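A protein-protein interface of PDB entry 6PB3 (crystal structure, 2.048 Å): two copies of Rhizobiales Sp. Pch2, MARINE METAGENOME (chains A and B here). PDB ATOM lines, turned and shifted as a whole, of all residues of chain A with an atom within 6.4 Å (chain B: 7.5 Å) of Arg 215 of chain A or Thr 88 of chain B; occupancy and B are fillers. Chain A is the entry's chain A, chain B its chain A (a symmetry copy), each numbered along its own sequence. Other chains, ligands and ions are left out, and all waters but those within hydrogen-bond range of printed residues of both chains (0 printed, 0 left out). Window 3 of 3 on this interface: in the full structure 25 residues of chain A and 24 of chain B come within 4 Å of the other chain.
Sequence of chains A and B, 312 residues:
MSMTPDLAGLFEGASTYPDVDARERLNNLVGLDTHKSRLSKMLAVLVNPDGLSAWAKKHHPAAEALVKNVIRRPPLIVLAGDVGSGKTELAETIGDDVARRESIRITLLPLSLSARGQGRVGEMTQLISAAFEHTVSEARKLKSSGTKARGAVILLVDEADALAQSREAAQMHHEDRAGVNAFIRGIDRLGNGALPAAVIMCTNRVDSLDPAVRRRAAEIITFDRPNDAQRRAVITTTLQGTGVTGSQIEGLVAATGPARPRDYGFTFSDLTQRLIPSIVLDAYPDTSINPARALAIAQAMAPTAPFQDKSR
NE2 of Gln 273 of chain B lies within hydrogen-bond range of O of Arg 214 of chain A (2.9 Å).
NE2 of Gln 273 of chain B is in hydrogen-bond range of O of Ala 217 of chain A (2.9 Å).
NH2 of Arg 73 of chain A is in hydrogen-bond range of O of Arg 215 of chain A (3.2 Å).
The backbone carbonyl oxygen (O) of Ala 217 of chain A sits at hydrogen-bond distance from the guanidinium group (NH2) of Arg 73 of chain A (2.9 Å).
The backbone carbonyl oxygen (O) of Ala 218 of chain A lies within hydrogen-bond range of the guanidinium group (NH1) of Arg 73 of chain A (3.4 Å).
OG of Ser 269 of chain B sits at hydrogen-bond distance from OE1 of Gln 273 of chain B (2.6 Å).
Among the printed residues, merely in contact across the chains: Arg 73 of chain A with Gln 273 of chain B, Pro 211 of chain A with Val 83 of chain B, Pro 211 of chain A with Asn 204 of chain B, Arg 214 of chain A with Val 83 of chain B, Arg 215 of chain A with Thr 88 of chain B and Arg 215 of chain A with Gln 273 of chain B.
Of chain B, only Thr 88 and Gln 273 come within 4 Å of Arg 215 of chain A.
Thr 88 of chain B touches one residue of chain A.
Of the printed residues of chain A, Val 83 of chain B touches Pro 211 (3.7 Å) and Arg 214 (3.8 Å).
Of the printed residues of chain B, Pro 211 of chain A touches Val 83 and Asn 204.
The nearest printed residue of chain A that does not touch Asn 204 of chain B is Arg 214 of chain A (5.8 Å).
Of the 12 printed residues of chain A, 5 touch a printed residue of chain B.
Printed residues of chain A that touch a printed residue of chain B: Arg 73, Pro 211, Arg 214, Arg 215 and Ala 217.
Hydrophobic or aromatic side chains of chain A that line the printed part of chain B: Pro 211 and Ala 217.
Among the printed residues, 8 pairs touch across the chains.
Among the printed residues, no Asp or Glu carboxylate lies within 4 Å of a Lys or Arg side-chain nitrogen of the other chain.
No position is printed for both chains.
Of the 8 pairs that touch across the chains among the printed residues, none has its exchanged pair printed and touching as well.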
ATOM      1  N   ARG A  73      -6.683  10.031 -37.425  1.00  0.00           N
ATOM      2  CA  ARG A  73      -7.155   9.189 -36.336  1.00  0.00           C
ATOM      3  C   ARG A  73      -7.622   7.832 -36.858  1.00  0.00           C
ATOM      4  O   ARG A  73      -8.235   7.749 -37.922  1.00  0.00           O
ATOM      5  CB  ARG A  73      -8.318   9.849 -35.608  1.00  0.00           C
ATOM      6  CG  ARG A  73      -8.087  11.255 -35.151  1.00  0.00           C
ATOM      7  CD  ARG A  73      -6.895  11.347 -34.194  1.00  0.00           C
ATOM      8  NE  ARG A  73      -6.787  10.256 -33.223  1.00  0.00           N
ATOM      9  CZ  ARG A  73      -7.537  10.137 -32.132  1.00  0.00           C
ATOM     10  NH1 ARG A  73      -8.494  11.027 -31.877  1.00  0.00           N
ATOM     11  NH2 ARG A  73      -7.333   9.122 -31.298  1.00  0.00           N
ATOM     12  N   PRO A  74      -7.397   6.761 -36.099  1.00  0.00           N
ATOM     13  CA  PRO A  74      -8.024   5.484 -36.446  1.00  0.00           C
ATOM     14  C   PRO A  74      -9.517   5.651 -36.579  1.00  0.00           C
ATOM     15  O   PRO A  74     -10.141   6.448 -35.850  1.00  0.00           O
ATOM     16  CB  PRO A  74      -7.658   4.580 -35.258  1.00  0.00           C
ATOM     17  CG  PRO A  74      -6.540   5.277 -34.542  1.00  0.00           C
ATOM     18  CD  PRO A  74      -6.769   6.741 -34.772  1.00  0.00           C
ATOM     19  N   ILE A 184      -8.333  -4.291 -31.748  1.00  0.00           N
ATOM     20  CA  ILE A 184      -7.297  -3.284 -31.970  1.00  0.00           C
ATOM     21  C   ILE A 184      -6.627  -3.496 -33.319  1.00  0.00           C
ATOM     22  O   ILE A 184      -6.448  -2.556 -34.102  1.00  0.00           O
ATOM     23  CB  ILE A 184      -6.260  -3.348 -30.838  1.00  0.00           C
ATOM     24  CG1 ILE A 184      -6.822  -2.770 -29.546  1.00  0.00           C
ATOM     25  CG2 ILE A 184      -4.967  -2.687 -31.245  1.00  0.00           C
ATOM     26  CD1 ILE A 184      -6.078  -3.318 -28.358  1.00  0.00           C
ATOM     27  N   ASP A 210     -11.713  -1.066 -22.741  1.00  0.00           N
ATOM     28  CA  ASP A 210     -10.277  -1.239 -22.621  1.00  0.00           C
ATOM     29  C   ASP A 210      -9.557   0.045 -23.043  1.00  0.00           C
ATOM     30  O   ASP A 210      -9.966   0.700 -24.004  1.00  0.00           O
ATOM     31  CB  ASP A 210      -9.801  -2.413 -23.474  1.00  0.00           C
ATOM     32  CG  ASP A 210      -8.338  -2.749 -23.221  1.00  0.00           C
ATOM     33  OD1 ASP A 210      -7.449  -1.990 -23.676  1.00  0.00           O
ATOM     34  OD2 ASP A 210      -8.078  -3.754 -22.530  1.00  0.00           O
ATOM     35  N   PRO A 211      -8.508   0.445 -22.323  1.00  0.00           N
ATOM     36  CA  PRO A 211      -7.817   1.707 -22.654  1.00  0.00           C
ATOM     37  C   PRO A 211      -7.257   1.733 -24.062  1.00  0.00           C
ATOM     38  O   PRO A 211      -7.256   2.786 -24.715  1.00  0.00           O
ATOM     39  CB  PRO A 211      -6.689   1.768 -21.613  1.00  0.00           C
ATOM     40  CG  PRO A 211      -7.141   0.853 -20.512  1.00  0.00           C
ATOM     41  CD  PRO A 211      -7.954  -0.213 -21.131  1.00  0.00           C
ATOM     42  N   ALA A 212      -6.760   0.595 -24.542  1.00  0.00           N
ATOM     43  CA  ALA A 212      -6.221   0.525 -25.895  1.00  0.00           C
ATOM     44  C   ALA A 212      -7.307   0.676 -26.952  1.00  0.00           C
ATOM     45  O   ALA A 212      -7.012   1.052 -28.098  1.00  0.00           O
ATOM     46  CB  ALA A 212      -5.460  -0.790 -26.069  1.00  0.00           C
ATOM     47  N   VAL A 213      -8.565   0.429 -26.582  1.00  0.00           N
ATOM     48  CA  VAL A 213      -9.664   0.777 -27.466  1.00  0.00           C
ATOM     49  C   VAL A 213      -9.980   2.258 -27.351  1.00  0.00           C
ATOM     50  O   VAL A 213     -10.126   2.951 -28.360  1.00  0.00           O
ATOM     51  CB  VAL A 213     -10.898  -0.091 -27.162  1.00  0.00           C
ATOM     52  CG1 VAL A 213     -12.150   0.506 -27.806  1.00  0.00           C
ATOM     53  CG2 VAL A 213     -10.665  -1.514 -27.642  1.00  0.00           C
ATOM     54  N   ARG A 214     -10.061   2.767 -26.121  1.00  0.00           N
ATOM     55  CA  ARG A 214     -10.477   4.150 -25.906  1.00  0.00           C
ATOM     56  C   ARG A 214      -9.544   5.126 -26.604  1.00  0.00           C
ATOM     57  O   ARG A 214      -9.997   6.077 -27.252  1.00  0.00           O
ATOM     58  CB  ARG A 214     -10.521   4.441 -24.408  1.00  0.00           C
ATOM     59  CG  ARG A 214     -11.682   5.291 -23.997  1.00  0.00           C
ATOM     60  CD  ARG A 214     -11.610   5.660 -22.547  1.00  0.00           C
ATOM     61  NE  ARG A 214     -11.369   4.504 -21.691  1.00  0.00           N
ATOM     62  CZ  ARG A 214     -11.234   4.603 -20.376  1.00  0.00           C
ATOM     63  NH1 ARG A 214     -11.331   5.800 -19.816  1.00  0.00           N
ATOM     64  NH2 ARG A 214     -11.004   3.527 -19.625  1.00  0.00           N
ATOM     65  N   ARG A 215      -8.235   4.896 -26.495  1.00  0.00           N
ATOM     66  CA  ARG A 215      -7.265   5.852 -27.011  1.00  0.00           C
ATOM     67  C   ARG A 215      -7.247   5.908 -28.530  1.00  0.00           C
ATOM     68  O   ARG A 215      -6.728   6.878 -29.085  1.00  0.00           O
ATOM     69  CB  ARG A 215      -5.866   5.519 -26.477  1.00  0.00           C
ATOM     70  CG  ARG A 215      -5.182   4.328 -27.137  1.00  0.00           C
ATOM     71  CD  ARG A 215      -3.767   4.121 -26.527  1.00  0.00           C
ATOM     72  NE  ARG A 215      -2.997   3.109 -27.250  1.00  0.00           N
ATOM     73  CZ  ARG A 215      -2.644   1.931 -26.742  1.00  0.00           C
ATOM     74  NH1 ARG A 215      -2.970   1.612 -25.486  1.00  0.00           N
ATOM     75  NH2 ARG A 215      -1.943   1.076 -27.482  1.00  0.00           N
ATOM     76  N   ARG A 216      -7.830   4.921 -29.205  1.00  0.00           N
ATOM     77  CA  ARG A 216      -7.924   4.914 -30.659  1.00  0.00           C
ATOM     78  C   ARG A 216      -9.173   5.600 -31.209  1.00  0.00           C
ATOM     79  O   ARG A 216      -9.232   5.849 -32.416  1.00  0.00           O
ATOM     80  CB  ARG A 216      -7.873   3.480 -31.175  1.00  0.00           C
ATOM     81  CG  ARG A 216      -6.478   2.880 -31.094  1.00  0.00           C
ATOM     82  CD  ARG A 216      -6.485   1.403 -31.429  1.00  0.00           C
ATOM     83  NE  ARG A 216      -5.132   0.886 -31.664  1.00  0.00           N
ATOM     84  CZ  ARG A 216      -4.289   0.514 -30.701  1.00  0.00           C
ATOM     85  NH1 ARG A 216      -4.638   0.627 -29.424  1.00  0.00           N
ATOM     86  NH2 ARG A 216      -3.089   0.028 -31.018  1.00  0.00           N
ATOM     87  N   ALA A 217     -10.152   5.931 -30.372  1.00  0.00           N
ATOM     88  CA  ALA A 217     -11.342   6.610 -30.871  1.00  0.00           C
ATOM     89  C   ALA A 217     -10.955   7.922 -31.547  1.00  0.00           C
ATOM     90  O   ALA A 217     -10.234   8.750 -30.974  1.00  0.00           O
ATOM     91  CB  ALA A 217     -12.332   6.874 -29.724  1.00  0.00           C
ATOM     92  N   ALA A 218     -11.406   8.088 -32.786  1.00  0.00           N
ATOM     93  CA  ALA A 218     -11.271   9.375 -33.446  1.00  0.00           C
ATOM     94  C   ALA A 218     -12.153  10.398 -32.771  1.00  0.00           C
ATOM     95  O   ALA A 218     -11.771  11.560 -32.626  1.00  0.00           O
ATOM     96  CB  ALA A 218     -11.639   9.257 -34.919  1.00  0.00           C
ATOM     97  N   ARG B  25       4.480  12.393 -35.712  1.00  0.00           N
ATOM     98  CA  ARG B  25       3.587  12.035 -34.613  1.00  0.00           C
ATOM     99  C   ARG B  25       3.951  12.778 -33.330  1.00  0.00           C
ATOM    100  O   ARG B  25       3.068  13.299 -32.643  1.00  0.00           O
ATOM    101  CB  ARG B  25       3.596  10.515 -34.396  1.00  0.00           C
ATOM    102  CG  ARG B  25       3.077   9.669 -35.623  1.00  0.00           C
ATOM    103  CD  ARG B  25       2.479   8.316 -35.153  1.00  0.00           C
ATOM    104  NE  ARG B  25       3.389   7.173 -35.218  1.00  0.00           N
ATOM    105  CZ  ARG B  25       3.456   6.199 -34.312  1.00  0.00           C
ATOM    106  NH1 ARG B  25       2.691   6.223 -33.231  1.00  0.00           N
ATOM    107  NH2 ARG B  25       4.310   5.200 -34.479  1.00  0.00           N
ATOM    108  N   LEU B  29       1.595  15.757 -31.054  1.00  0.00           N
ATOM    109  CA  LEU B  29       1.235  15.764 -29.638  1.00  0.00           C
ATOM    110  C   LEU B  29       1.372  17.172 -29.075  1.00  0.00           C
ATOM    111  O   LEU B  29       2.483  17.704 -28.992  1.00  0.00           O
ATOM    112  CB  LEU B  29       2.117  14.806 -28.845  1.00  0.00           C
ATOM    113  CG  LEU B  29       2.072  13.339 -29.254  1.00  0.00           C
ATOM    114  CD1 LEU B  29       2.904  12.505 -28.277  1.00  0.00           C
ATOM    115  CD2 LEU B  29       0.643  12.843 -29.273  1.00  0.00           C
ATOM    116  N   LEU B  79       5.178   5.847 -17.237  1.00  0.00           N
ATOM    117  CA  LEU B  79       4.212   6.849 -17.679  1.00  0.00           C
ATOM    118  C   LEU B  79       2.863   6.457 -17.114  1.00  0.00           C
ATOM    119  O   LEU B  79       2.330   5.402 -17.468  1.00  0.00           O
ATOM    120  CB  LEU B  79       4.148   6.940 -19.211  1.00  0.00           C
ATOM    121  CG  LEU B  79       5.435   7.118 -20.011  1.00  0.00           C
ATOM    122  CD1 LEU B  79       5.088   7.437 -21.490  1.00  0.00           C
ATOM    123  CD2 LEU B  79       6.303   8.205 -19.421  1.00  0.00           C
ATOM    124  N   VAL B  83      -6.320   7.701 -19.316  1.00  0.00           N
ATOM    125  CA  VAL B  83      -6.397   7.055 -20.615  1.00  0.00           C
ATOM    126  C   VAL B  83      -6.649   8.096 -21.695  1.00  0.00           C
ATOM    127  O   VAL B  83      -7.407   9.056 -21.500  1.00  0.00           O
ATOM    128  CB  VAL B  83      -7.506   5.994 -20.586  1.00  0.00           C
ATOM    129  CG1 VAL B  83      -7.651   5.331 -21.946  1.00  0.00           C
ATOM    130  CG2 VAL B  83      -7.217   4.972 -19.496  1.00  0.00           C
ATOM    131  N   GLY B  84      -6.016   7.903 -22.850  1.00  0.00           N
ATOM    132  CA  GLY B  84      -6.239   8.802 -23.964  1.00  0.00           C
ATOM    133  C   GLY B  84      -5.486  10.107 -23.874  1.00  0.00           C
ATOM    134  O   GLY B  84      -5.825  11.051 -24.594  1.00  0.00           O
ATOM    135  N   SER B  85      -4.516  10.206 -22.972  1.00  0.00           N
ATOM    136  CA  SER B  85      -3.668  11.383 -22.874  1.00  0.00           C
ATOM    137  C   SER B  85      -2.563  11.415 -23.924  1.00  0.00           C
ATOM    138  O   SER B  85      -1.934  12.462 -24.089  1.00  0.00           O
ATOM    139  CB  SER B  85      -3.025  11.451 -21.488  1.00  0.00           C
ATOM    140  OG  SER B  85      -4.005  11.426 -20.474  1.00  0.00           O
ATOM    141  N   GLY B  86      -2.308  10.311 -24.624  1.00  0.00           N
ATOM    142  CA  GLY B  86      -1.175  10.227 -25.536  1.00  0.00           C
ATOM    143  C   GLY B  86       0.057   9.547 -24.971  1.00  0.00           C
ATOM    144  O   GLY B  86       1.134   9.619 -25.597  1.00  0.00           O
ATOM    145  N   LYS B  87      -0.065   8.889 -23.816  1.00  0.00           N
ATOM    146  CA  LYS B  87       1.081   8.226 -23.191  1.00  0.00           C
ATOM    147  C   LYS B  87       1.724   7.226 -24.139  1.00  0.00           C
ATOM    148  O   LYS B  87       2.948   7.224 -24.328  1.00  0.00           O
ATOM    149  CB  LYS B  87       0.640   7.511 -21.906  1.00  0.00           C
ATOM    150  CG  LYS B  87       0.098   8.415 -20.809  1.00  0.00           C
ATOM    151  CD  LYS B  87      -0.204   7.609 -19.545  1.00  0.00           C
ATOM    152  CE  LYS B  87      -1.611   6.982 -19.573  1.00  0.00           C
ATOM    153  NZ  LYS B  87      -1.725   5.761 -20.403  1.00  0.00           N
ATOM    154  N   THR B  88       0.908   6.336 -24.711  1.00  0.00           N
ATOM    155  CA  THR B  88       1.420   5.312 -25.616  1.00  0.00           C
ATOM    156  C   THR B  88       2.028   5.945 -26.858  1.00  0.00           C
ATOM    157  O   THR B  88       3.126   5.575 -27.292  1.00  0.00           O
ATOM    158  CB  THR B  88       0.281   4.363 -26.002  1.00  0.00           C
ATOM    159  OG1 THR B  88      -0.364   3.893 -24.812  1.00  0.00           O
ATOM    160  CG2 THR B  88       0.803   3.182 -26.819  1.00  0.00           C
ATOM    161  N   GLU B  89       1.310   6.902 -27.452  1.00  0.00           N
ATOM    162  CA  GLU B  89       1.814   7.565 -28.644  1.00  0.00           C
ATOM    163  C   GLU B  89       3.114   8.293 -28.339  1.00  0.00           C
ATOM    164  O   GLU B  89       4.035   8.308 -29.163  1.00  0.00           O
ATOM    165  CB  GLU B  89       0.753   8.521 -29.191  1.00  0.00           C
ATOM    166  CG  GLU B  89       1.193   9.315 -30.406  1.00  0.00           C
ATOM    167  CD  GLU B  89       0.998   8.561 -31.704  1.00  0.00           C
ATOM    168  OE1 GLU B  89       0.802   7.325 -31.660  1.00  0.00           O
ATOM    169  OE2 GLU B  89       1.039   9.214 -32.770  1.00  0.00           O
ATOM    170  N   LEU B  90       3.225   8.871 -27.142  1.00  0.00           N
ATOM    171  CA  LEU B  90       4.491   9.488 -26.753  1.00  0.00           C
ATOM    172  C   LEU B  90       5.592   8.441 -26.609  1.00  0.00           C
ATOM    173  O   LEU B  90       6.703   8.619 -27.123  1.00  0.00           O
ATOM    174  CB  LEU B  90       4.309  10.268 -25.450  1.00  0.00           C
ATOM    175  CG  LEU B  90       5.564  10.955 -24.918  1.00  0.00           C
ATOM    176  CD1 LEU B  90       6.042  12.027 -25.915  1.00  0.00           C
ATOM    177  CD2 LEU B  90       5.300  11.571 -23.571  1.00  0.00           C
ATOM    178  N   ALA B  91       5.297   7.327 -25.937  1.00  0.00           N
ATOM    179  CA  ALA B  91       6.329   6.322 -25.722  1.00  0.00           C
ATOM    180  C   ALA B  91       6.791   5.701 -27.032  1.00  0.00           C
ATOM    181  O   ALA B  91       7.956   5.308 -27.147  1.00  0.00           O
ATOM    182  CB  ALA B  91       5.815   5.240 -24.765  1.00  0.00           C
ATOM    183  N   GLU B  92       5.894   5.579 -28.013  1.00  0.00           N
ATOM    184  CA  GLU B  92       6.240   4.958 -29.286  1.00  0.00           C
ATOM    185  C   GLU B  92       7.005   5.880 -30.212  1.00  0.00           C
ATOM    186  O   GLU B  92       7.537   5.406 -31.219  1.00  0.00           O
ATOM    187  CB  GLU B  92       4.983   4.489 -30.012  1.00  0.00           C
ATOM    188  CG  GLU B  92       4.279   3.305 -29.368  1.00  0.00           C
ATOM    189  CD  GLU B  92       3.040   2.913 -30.157  1.00  0.00           C
ATOM    190  OE1 GLU B  92       2.613   3.716 -31.015  1.00  0.00           O
ATOM    191  OE2 GLU B  92       2.493   1.812 -29.926  1.00  0.00           O
ATOM    192  N   THR B  93       7.053   7.177 -29.929  1.00  0.00           N
ATOM    193  CA  THR B  93       7.727   8.101 -30.829  1.00  0.00           C
ATOM    194  C   THR B  93       8.880   8.868 -30.196  1.00  0.00           C
ATOM    195  O   THR B  93       9.712   9.407 -30.936  1.00  0.00           O
ATOM    196  CB  THR B  93       6.721   9.108 -31.407  1.00  0.00           C
ATOM    197  OG1 THR B  93       6.068   9.810 -30.339  1.00  0.00           O
ATOM    198  CG2 THR B  93       5.685   8.378 -32.240  1.00  0.00           C
ATOM    199  N   ILE B  94       8.965   8.905 -28.862  1.00  0.00           N
ATOM    200  CA  ILE B  94       9.936   9.736 -28.157  1.00  0.00           C
ATOM    201  C   ILE B  94      11.370   9.367 -28.500  1.00  0.00           C
ATOM    202  O   ILE B  94      12.277  10.192 -28.329  1.00  0.00           O
ATOM    203  CB  ILE B  94       9.685   9.637 -26.634  1.00  0.00           C
ATOM    204  CG1 ILE B  94      10.363  10.783 -25.884  1.00  0.00           C
ATOM    205  CG2 ILE B  94      10.129   8.275 -26.089  1.00  0.00           C
ATOM    206  CD1 ILE B  94       9.968  12.152 -26.419  1.00  0.00           C
ATOM    207  N   LEU B 156       9.690  -1.312 -24.658  1.00  0.00           N
ATOM    208  CA  LEU B 156       8.412  -0.686 -24.339  1.00  0.00           C
ATOM    209  C   LEU B 156       7.410  -1.744 -23.897  1.00  0.00           C
ATOM    210  O   LEU B 156       7.227  -2.755 -24.587  1.00  0.00           O
ATOM    211  CB  LEU B 156       7.881   0.092 -25.551  1.00  0.00           C
ATOM    212  CG  LEU B 156       6.510   0.770 -25.463  1.00  0.00           C
ATOM    213  CD1 LEU B 156       6.271   1.482 -24.126  1.00  0.00           C
ATOM    214  CD2 LEU B 156       6.342   1.758 -26.636  1.00  0.00           C
ATOM    215  N   VAL B 157       6.748  -1.489 -22.767  1.00  0.00           N
ATOM    216  CA  VAL B 157       5.769  -2.393 -22.165  1.00  0.00           C
ATOM    217  C   VAL B 157       4.434  -1.661 -22.019  1.00  0.00           C
ATOM    218  O   VAL B 157       4.340  -0.676 -21.271  1.00  0.00           O
ATOM    219  CB  VAL B 157       6.242  -2.906 -20.795  1.00  0.00           C
ATOM    220  CG1 VAL B 157       5.340  -4.018 -20.323  1.00  0.00           C
ATOM    221  CG2 VAL B 157       7.693  -3.365 -20.853  1.00  0.00           C
ATOM    222  N   ASP B 158       3.393  -2.173 -22.688  1.00  0.00           N
ATOM    223  CA  ASP B 158       2.072  -1.544 -22.724  1.00  0.00           C
ATOM    224  C   ASP B 158       1.144  -2.006 -21.605  1.00  0.00           C
ATOM    225  O   ASP B 158       0.101  -1.375 -21.386  1.00  0.00           O
ATOM    226  CB  ASP B 158       1.399  -1.809 -24.076  1.00  0.00           C
ATOM    227  N   ILE B 200      10.478   1.588 -20.881  1.00  0.00           N
ATOM    228  CA  ILE B 200       9.347   2.482 -20.695  1.00  0.00           C
ATOM    229  C   ILE B 200       8.133   1.622 -20.424  1.00  0.00           C
ATOM    230  O   ILE B 200       7.828   0.694 -21.189  1.00  0.00           O
ATOM    231  CB  ILE B 200       9.093   3.370 -21.929  1.00  0.00           C
ATOM    232  CG1 ILE B 200      10.321   4.228 -22.239  1.00  0.00           C
ATOM    233  CG2 ILE B 200       7.812   4.208 -21.712  1.00  0.00           C
ATOM    234  CD1 ILE B 200      10.250   4.967 -23.568  1.00  0.00           C
ATOM    235  N   CYS B 202       3.883   1.934 -19.543  1.00  0.00           N
ATOM    236  CA  CYS B 202       2.709   2.776 -19.422  1.00  0.00           C
ATOM    237  C   CYS B 202       1.682   2.068 -18.557  1.00  0.00           C
ATOM    238  O   CYS B 202       1.509   0.849 -18.656  1.00  0.00           O
ATOM    239  CB  CYS B 202       2.103   3.099 -20.812  1.00  0.00           C
ATOM    240  SG  CYS B 202       3.281   3.891 -21.933  1.00  0.00           S
ATOM    241  N   THR B 203       0.991   2.843 -17.725  1.00  0.00           N
ATOM    242  CA  THR B 203      -0.085   2.347 -16.888  1.00  0.00           C
ATOM    243  C   THR B 203      -1.104   3.465 -16.742  1.00  0.00           C
ATOM    244  O   THR B 203      -0.758   4.649 -16.781  1.00  0.00           O
ATOM    245  CB  THR B 203       0.426   1.903 -15.516  1.00  0.00           C
ATOM    246  OG1 THR B 203      -0.655   1.357 -14.764  1.00  0.00           O
ATOM    247  CG2 THR B 203       1.016   3.084 -14.762  1.00  0.00           C
ATOM    248  N   ASN B 204      -2.366   3.087 -16.605  1.00  0.00           N
ATOM    249  CA  ASN B 204      -3.390   4.091 -16.358  1.00  0.00           C
ATOM    250  C   ASN B 204      -3.297   4.611 -14.935  1.00  0.00           C
ATOM    251  O   ASN B 204      -3.281   5.825 -14.706  1.00  0.00           O
ATOM    252  CB  ASN B 204      -4.767   3.506 -16.636  1.00  0.00           C
ATOM    253  CG  ASN B 204      -4.842   2.887 -17.992  1.00  0.00           C
ATOM    254  OD1 ASN B 204      -4.144   3.308 -18.925  1.00  0.00           O
ATOM    255  ND2 ASN B 204      -5.666   1.862 -18.117  1.00  0.00           N
ATOM    256  N   PHE B 223       0.458  12.011 -16.190  1.00  0.00           N
ATOM    257  CA  PHE B 223      -0.452  12.576 -17.177  1.00  0.00           C
ATOM    258  C   PHE B 223      -1.796  12.717 -16.472  1.00  0.00           C
ATOM    259  O   PHE B 223      -2.631  11.808 -16.471  1.00  0.00           O
ATOM    260  CB  PHE B 223      -0.557  11.688 -18.423  1.00  0.00           C
ATOM    261  CG  PHE B 223       0.755  11.477 -19.128  1.00  0.00           C
ATOM    262  CD1 PHE B 223       1.754  10.723 -18.543  1.00  0.00           C
ATOM    263  CD2 PHE B 223       0.992  12.045 -20.371  1.00  0.00           C
ATOM    264  CE1 PHE B 223       2.977  10.544 -19.178  1.00  0.00           C
ATOM    265  CE2 PHE B 223       2.212  11.863 -21.018  1.00  0.00           C
ATOM    266  CZ  PHE B 223       3.197  11.107 -20.428  1.00  0.00           C
ATOM    267  N   SER B 269      -7.840  13.743 -23.097  1.00  0.00           N
ATOM    268  CA  SER B 269      -8.819  13.079 -23.957  1.00  0.00           C
ATOM    269  C   SER B 269     -10.029  13.961 -24.235  1.00  0.00           C
ATOM    270  O   SER B 269     -10.490  14.045 -25.381  1.00  0.00           O
ATOM    271  CB  SER B 269      -9.269  11.777 -23.307  1.00  0.00           C
ATOM    272  OG  SER B 269     -10.180  11.119 -24.152  1.00  0.00           O
ATOM    273  N   THR B 272      -8.900  16.342 -26.964  1.00  0.00           N
ATOM    274  CA  THR B 272      -8.481  15.870 -28.280  1.00  0.00           C
ATOM    275  C   THR B 272      -9.512  14.966 -28.931  1.00  0.00           C
ATOM    276  O   THR B 272      -9.648  14.989 -30.157  1.00  0.00           O
ATOM    277  CB  THR B 272      -7.135  15.129 -28.195  1.00  0.00           C
ATOM    278  OG1 THR B 272      -7.236  14.005 -27.301  1.00  0.00           O
ATOM    279  CG2 THR B 272      -6.010  16.055 -27.693  1.00  0.00           C
ATOM    280  N   GLN B 273     -10.246  14.174 -28.146  1.00  0.00           N
ATOM    281  CA  GLN B 273     -11.209  13.224 -28.699  1.00  0.00           C
ATOM    282  C   GLN B 273     -12.659  13.694 -28.622  1.00  0.00           C
ATOM    283  O   GLN B 273     -13.536  13.044 -29.218  1.00  0.00           O
ATOM    284  CB  GLN B 273     -11.070  11.869 -27.986  1.00  0.00           C
ATOM    285  CG  GLN B 273      -9.667  11.205 -28.179  1.00  0.00           C
ATOM    286  CD  GLN B 273      -9.571   9.888 -27.429  1.00  0.00           C
ATOM    287  OE1 GLN B 273      -9.333   9.872 -26.225  1.00  0.00           O
ATOM    288  NE2 GLN B 273      -9.797   8.787 -28.124  1.00  0.00           N
